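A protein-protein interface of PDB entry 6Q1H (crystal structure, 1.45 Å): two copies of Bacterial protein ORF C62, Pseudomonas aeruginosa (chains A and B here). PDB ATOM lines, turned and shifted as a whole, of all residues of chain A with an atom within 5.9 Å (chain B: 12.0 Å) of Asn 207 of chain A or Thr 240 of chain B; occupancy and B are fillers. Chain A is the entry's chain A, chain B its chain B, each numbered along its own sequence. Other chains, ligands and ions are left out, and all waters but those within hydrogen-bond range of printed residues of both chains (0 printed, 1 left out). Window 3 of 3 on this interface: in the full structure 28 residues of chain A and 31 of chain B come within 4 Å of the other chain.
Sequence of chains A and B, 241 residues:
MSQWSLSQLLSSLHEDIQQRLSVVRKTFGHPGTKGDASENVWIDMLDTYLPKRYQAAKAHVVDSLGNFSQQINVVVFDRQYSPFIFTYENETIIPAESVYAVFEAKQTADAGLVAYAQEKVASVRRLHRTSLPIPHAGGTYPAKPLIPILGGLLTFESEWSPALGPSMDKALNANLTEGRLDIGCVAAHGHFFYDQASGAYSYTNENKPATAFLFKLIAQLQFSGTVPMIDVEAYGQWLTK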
ATOM      1  N   THR A 204      20.288  18.855   4.297  1.00  0.00           N
ATOM      2  CA  THR A 204      20.106  17.852   5.338  1.00  0.00           C
ATOM      3  C   THR A 204      20.009  18.582   6.662  1.00  0.00           C
ATOM      4  O   THR A 204      20.953  19.271   7.064  1.00  0.00           O
ATOM      5  CB  THR A 204      21.274  16.862   5.339  1.00  0.00           C
ATOM      6  OG1 THR A 204      21.388  16.257   4.040  1.00  0.00           O
ATOM      7  CG2 THR A 204      21.044  15.773   6.382  1.00  0.00           C
ATOM      8  N   ASN A 205      18.874  18.444   7.327  1.00  0.00           N
ATOM      9  CA  ASN A 205      18.659  19.034   8.636  1.00  0.00           C
ATOM     10  C   ASN A 205      19.075  18.057   9.727  1.00  0.00           C
ATOM     11  O   ASN A 205      18.912  16.844   9.586  1.00  0.00           O
ATOM     12  CB  ASN A 205      17.193  19.421   8.778  1.00  0.00           C
ATOM     13  CG  ASN A 205      16.792  20.507   7.791  1.00  0.00           C
ATOM     14  OD1 ASN A 205      17.192  21.649   7.936  1.00  0.00           O
ATOM     15  ND2 ASN A 205      16.032  20.140   6.766  1.00  0.00           N
ATOM     16  N   GLU A 206      19.615  18.604  10.811  1.00  0.00           N
ATOM     17  CA  GLU A 206      20.110  17.796  11.949  1.00  0.00           C
ATOM     18  C   GLU A 206      21.129  16.788  11.409  1.00  0.00           C
ATOM     19  O   GLU A 206      21.974  17.156  10.580  1.00  0.00           O
ATOM     20  CB  GLU A 206      18.919  17.241  12.714  1.00  0.00           C
ATOM     21  CG  GLU A 206      18.014  18.347  13.276  1.00  0.00           C
ATOM     22  CD  GLU A 206      16.836  17.827  14.094  1.00  0.00           C
ATOM     23  OE1 GLU A 206      15.999  17.090  13.537  1.00  0.00           O
ATOM     24  OE2 GLU A 206      16.753  18.166  15.293  1.00  0.00           O
ATOM     25  N   ASN A 207      21.107  15.537  11.870  1.00  0.00           N
ATOM     26  CA  ASN A 207      22.057  14.518  11.421  1.00  0.00           C
ATOM     27  C   ASN A 207      23.502  14.936  11.687  1.00  0.00           C
ATOM     28  O   ASN A 207      24.398  14.682  10.872  1.00  0.00           O
ATOM     29  CB  ASN A 207      21.868  14.143   9.954  1.00  0.00           C
ATOM     30  CG  ASN A 207      20.628  13.326   9.720  1.00  0.00           C
ATOM     31  OD1 ASN A 207      19.956  12.899  10.662  1.00  0.00           O
ATOM     32  ND2 ASN A 207      20.320  13.087   8.449  1.00  0.00           N
ATOM     33  N   LYS A 208      23.724  15.597  12.829  1.00  0.00           N
ATOM     34  CA  LYS A 208      25.052  15.975  13.326  1.00  0.00           C
ATOM     35  C   LYS A 208      25.747  16.882  12.313  1.00  0.00           C
ATOM     36  O   LYS A 208      26.759  16.497  11.703  1.00  0.00           O
ATOM     37  CB  LYS A 208      25.878  14.728  13.666  1.00  0.00           C
ATOM     38  CG  LYS A 208      25.095  13.706  14.501  1.00  0.00           C
ATOM     39  CD  LYS A 208      25.717  12.321  14.389  1.00  0.00           C
ATOM     40  CE  LYS A 208      24.819  11.244  15.000  1.00  0.00           C
ATOM     41  NZ  LYS A 208      25.538   9.941  15.130  1.00  0.00           N
ATOM     42  N   PRO A 209      25.238  18.117  12.148  1.00  0.00           N
ATOM     43  CA  PRO A 209      25.669  18.952  11.014  1.00  0.00           C
ATOM     44  C   PRO A 209      27.155  19.137  10.796  1.00  0.00           C
ATOM     45  O   PRO A 209      27.592  19.111   9.655  1.00  0.00           O
ATOM     46  CB  PRO A 209      24.961  20.294  11.266  1.00  0.00           C
ATOM     47  CG  PRO A 209      23.834  19.994  12.143  1.00  0.00           C
ATOM     48  CD  PRO A 209      24.076  18.684  12.858  1.00  0.00           C
ATOM     49  N   THR A 211      29.715  17.249  11.676  1.00  0.00           N
ATOM     50  CA  THR A 211      30.312  16.000  11.210  1.00  0.00           C
ATOM     51  C   THR A 211      29.861  15.672   9.800  1.00  0.00           C
ATOM     52  O   THR A 211      30.651  15.203   8.971  1.00  0.00           O
ATOM     53  CB  THR A 211      29.940  14.855  12.139  1.00  0.00           C
ATOM     54  OG1 THR A 211      30.184  15.256  13.480  1.00  0.00           O
ATOM     55  CG2 THR A 211      30.803  13.604  11.820  1.00  0.00           C
ATOM     56  N   ALA A 212      28.566  15.865   9.523  1.00  0.00           N
ATOM     57  CA  ALA A 212      28.068  15.636   8.176  1.00  0.00           C
ATOM     58  C   ALA A 212      28.799  16.516   7.174  1.00  0.00           C
ATOM     59  O   ALA A 212      29.162  16.055   6.071  1.00  0.00           O
ATOM     60  CB  ALA A 212      26.561  15.860   8.122  1.00  0.00           C
ATOM     61  N   SER B  64      33.762   1.176   9.576  1.00  0.00           N
ATOM     62  CA  SER B  64      32.482   1.715   9.124  1.00  0.00           C
ATOM     63  C   SER B  64      31.314   0.779   9.380  1.00  0.00           C
ATOM     64  O   SER B  64      30.164   1.143   9.082  1.00  0.00           O
ATOM     65  CB  SER B  64      32.561   2.106   7.643  1.00  0.00           C
ATOM     66  OG  SER B  64      32.824   0.965   6.836  1.00  0.00           O
ATOM     67  N   VAL B 232      34.885   7.878   3.447  1.00  0.00           N
ATOM     68  CA  VAL B 232      34.390   8.452   4.686  1.00  0.00           C
ATOM     69  C   VAL B 232      32.868   8.444   4.758  1.00  0.00           C
ATOM     70  O   VAL B 232      32.312   8.455   5.854  1.00  0.00           O
ATOM     71  CB  VAL B 232      34.910   9.876   4.985  1.00  0.00           C
ATOM     72  CG1 VAL B 232      36.389   9.850   5.083  1.00  0.00           C
ATOM     73  CG2 VAL B 232      34.456  10.876   3.941  1.00  0.00           C
ATOM     74  N   GLU B 233      32.173   8.425   3.622  1.00  0.00           N
ATOM     75  CA  GLU B 233      30.712   8.389   3.666  1.00  0.00           C
ATOM     76  C   GLU B 233      30.176   7.046   4.140  1.00  0.00           C
ATOM     77  O   GLU B 233      29.012   6.979   4.563  1.00  0.00           O
ATOM     78  CB  GLU B 233      30.180   8.841   2.318  1.00  0.00           C
ATOM     79  CG  GLU B 233      30.529  10.325   2.094  1.00  0.00           C
ATOM     80  CD  GLU B 233      30.097  10.839   0.740  1.00  0.00           C
ATOM     81  OE1 GLU B 233      30.445  10.193  -0.264  1.00  0.00           O
ATOM     82  OE2 GLU B 233      29.417  11.890   0.690  1.00  0.00           O
ATOM     83  N   ALA B 234      30.992   5.991   4.119  1.00  0.00           N
ATOM     84  CA  ALA B 234      30.586   4.745   4.761  1.00  0.00           C
ATOM     85  C   ALA B 234      30.454   4.935   6.265  1.00  0.00           C
ATOM     86  O   ALA B 234      29.562   4.358   6.899  1.00  0.00           O
ATOM     87  CB  ALA B 234      31.595   3.638   4.444  1.00  0.00           C
ATOM     88  N   TYR B 235      31.329   5.755   6.845  1.00  0.00           N
ATOM     89  CA  TYR B 235      31.210   6.118   8.251  1.00  0.00           C
ATOM     90  C   TYR B 235      30.029   7.058   8.465  1.00  0.00           C
ATOM     91  O   TYR B 235      29.337   6.972   9.484  1.00  0.00           O
ATOM     92  CB  TYR B 235      32.515   6.774   8.732  1.00  0.00           C
ATOM     93  CG  TYR B 235      33.683   5.812   8.863  1.00  0.00           C
ATOM     94  CD1 TYR B 235      34.472   5.471   7.768  1.00  0.00           C
ATOM     95  CD2 TYR B 235      33.961   5.194  10.079  1.00  0.00           C
ATOM     96  CE1 TYR B 235      35.537   4.585   7.917  1.00  0.00           C
ATOM     97  CE2 TYR B 235      35.001   4.300  10.214  1.00  0.00           C
ATOM     98  CZ  TYR B 235      35.784   4.013   9.154  1.00  0.00           C
ATOM     99  OH  TYR B 235      36.790   3.108   9.303  1.00  0.00           O
ATOM    100  N   GLY B 236      29.770   7.927   7.490  1.00  0.00           N
ATOM    101  CA  GLY B 236      28.628   8.835   7.536  1.00  0.00           C
ATOM    102  C   GLY B 236      27.277   8.149   7.603  1.00  0.00           C
ATOM    103  O   GLY B 236      26.273   8.802   7.944  1.00  0.00           O
ATOM    104  N   GLN B 237      27.209   6.856   7.294  1.00  0.00           N
ATOM    105  CA  GLN B 237      25.932   6.167   7.457  1.00  0.00           C
ATOM    106  C   GLN B 237      25.478   6.144   8.912  1.00  0.00           C
ATOM    107  O   GLN B 237      24.292   5.926   9.174  1.00  0.00           O
ATOM    108  CB  GLN B 237      26.024   4.746   6.914  1.00  0.00           C
ATOM    109  CG  GLN B 237      26.403   4.663   5.426  1.00  0.00           C
ATOM    110  CD  GLN B 237      25.378   5.292   4.507  1.00  0.00           C
ATOM    111  OE1 GLN B 237      24.213   5.456   4.872  1.00  0.00           O
ATOM    112  NE2 GLN B 237      25.812   5.655   3.304  1.00  0.00           N
ATOM    113  N   TRP B 238      26.389   6.377   9.860  1.00  0.00           N
ATOM    114  CA  TRP B 238      26.083   6.346  11.281  1.00  0.00           C
ATOM    115  C   TRP B 238      25.690   7.709  11.822  1.00  0.00           C
ATOM    116  O   TRP B 238      25.519   7.847  13.039  1.00  0.00           O
ATOM    117  CB  TRP B 238      27.273   5.791  12.051  1.00  0.00           C
ATOM    118  CG  TRP B 238      27.560   4.395  11.663  1.00  0.00           C
ATOM    119  CD1 TRP B 238      28.328   3.967  10.610  1.00  0.00           C
ATOM    120  CD2 TRP B 238      27.037   3.219  12.272  1.00  0.00           C
ATOM    121  NE1 TRP B 238      28.333   2.600  10.550  1.00  0.00           N
ATOM    122  CE2 TRP B 238      27.547   2.112  11.555  1.00  0.00           C
ATOM    123  CE3 TRP B 238      26.190   2.989  13.357  1.00  0.00           C
ATOM    124  CZ2 TRP B 238      27.236   0.800  11.893  1.00  0.00           C
ATOM    125  CZ3 TRP B 238      25.895   1.684  13.697  1.00  0.00           C
ATOM    126  CH2 TRP B 238      26.418   0.609  12.969  1.00  0.00           C
ATOM    127  N   LEU B 239      25.570   8.709  10.941  1.00  0.00           N
ATOM    128  CA  LEU B 239      25.078  10.036  11.311  1.00  0.00           C
ATOM    129  C   LEU B 239      23.569  10.065  11.514  1.00  0.00           C
ATOM    130  O   LEU B 239      23.055  11.001  12.131  1.00  0.00           O
ATOM    131  CB  LEU B 239      25.359  11.037  10.183  1.00  0.00           C
ATOM    132  CG  LEU B 239      26.815  11.353   9.863  1.00  0.00           C
ATOM    133  CD1 LEU B 239      26.992  11.983   8.508  1.00  0.00           C
ATOM    134  CD2 LEU B 239      27.357  12.277  10.939  1.00  0.00           C
ATOM    135  N   THR B 240      22.854   9.096  10.956  1.00  0.00           N
ATOM    136  CA  THR B 240      21.405   9.003  11.076  1.00  0.00           C
ATOM    137  C   THR B 240      21.009   7.880  12.020  1.00  0.00           C
ATOM    138  O   THR B 240      19.830   7.515  12.084  1.00  0.00           O
ATOM    139  CB  THR B 240      20.790   8.769   9.695  1.00  0.00           C
ATOM    140  OG1 THR B 240      21.366   7.589   9.121  1.00  0.00           O
ATOM    141  CG2 THR B 240      21.042   9.960   8.767  1.00  0.00           C
ATOM    142  N   LYS B 241      21.981   7.319  12.738  1.00  0.00           N
ATOM    143  CA  LYS B 241      21.775   6.181  13.613  1.00  0.00           C
ATOM    144  C   LYS B 241      22.342   6.500  14.996  1.00  0.00           C
ATOM    145  O   LYS B 241      22.493   7.666  15.360  1.00  0.00           O
ATOM    146  CB  LYS B 241      22.506   4.947  13.085  1.00  0.00           C
ATOM    147  CG  LYS B 241      22.165   4.518  11.666  1.00  0.00           C
ATOM    148  CD  LYS B 241      22.335   2.996  11.543  1.00  0.00           C
ATOM    149  CE  LYS B 241      23.100   2.585  10.294  1.00  0.00           C
ATOM    150  NZ  LYS B 241      23.931   1.369  10.528  1.00  0.00           N
ATOM    151  OXT LYS B 241      22.686   5.585  15.748  1.00  0.00           O
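Of the 8 printed residues of chain A, 4 touch a printed residue of chain B. Printed residues of chain A that touch a printed residue of chain B: Asn 207, Lys 208, Thr 211 and Ala 212. Hydrophobic or aromatic side chains of chain A within 4 Å of the printed part of chain B: Ala 212. Hydrophobic or aromatic side chains of chain B within 4 Å of the printed part of chain A: Leu 239. Among the printed residues, 7 pairs touch across the chains. Among the printed residues, no Asp or Glu carboxylate lies within 4 Å of a Lys or Arg side-chain nitrogen of the other chain.
No residue of chain B comes within 4 Å of Thr 204 of chain A. Of chain B, only Leu 239 (3.7 Å) and Thr 240 (3.2 Å) come within 4 Å of Asn 207 of chain A. Lys 208 of chain A touches just these residues of chain B: Trp 238, Leu 239 and Lys 241. No residue of chain B comes within 4 Å of Pro 209 of chain A. Of chain B, only Leu 239 comes within 4 Å of Thr 211 of chain A. Of chain B, only Leu 239 comes within 4 Å of Ala 212 of chain A. Printed residues of chain A within 4 Å of Trp 238 of chain B: Lys 208. Of the printed residues of chain A, Leu 239 of chain B touches Asn 207 (3.7 Å), Lys 208 (3.4 Å), Thr 211 (3.8 Å) and Ala 212 (3.8 Å). Of chain A, only Asn 207 (3.2 Å) comes within 4 Å of Thr 240 of chain B. Printed residues of chain A within 4 Å of Lys 241 of chain B: Lys 208 (3.8 Å). The nearest printed residue of chain A that does not touch Lys 241 of chain B is Asn 207 of chain A (6.3 Å).
O of Ser 64 of chain B lies within hydrogen-bond range of NE1 of Trp 238 of chain B (2.8 Å). O of Gln 237 of chain B sits at hydrogen-bond distance from OG1 of Thr 240 of chain B, at 3.4 Å.
Asn 207 of chain A touches Leu 239 of chain B. Thr 240 of chain B touches Asn 207 of chain A. O of Leu 239 of chain B touches CE of Lys 208 of chain A, at 3.4 Å. Thr 211 of chain A touches Leu 239 of chain B (CG2 to CD2, 3.8 Å). CA of Ala 212 of chain A touches CD1 of Leu 239 of chain B, 3.8 Å away.
No position is printed for both chains. Of the 7 pairs that touch across the chains among the printed residues, none has its exchanged pair printed and touching as well.
NZ of Lys 208 of chain A is in hydrogen-bond range of O of Trp 238 of chain B (3.0 Å). NZ of Lys 208 of chain A is in salt-bridge range of O of Lys 241 of chain B.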
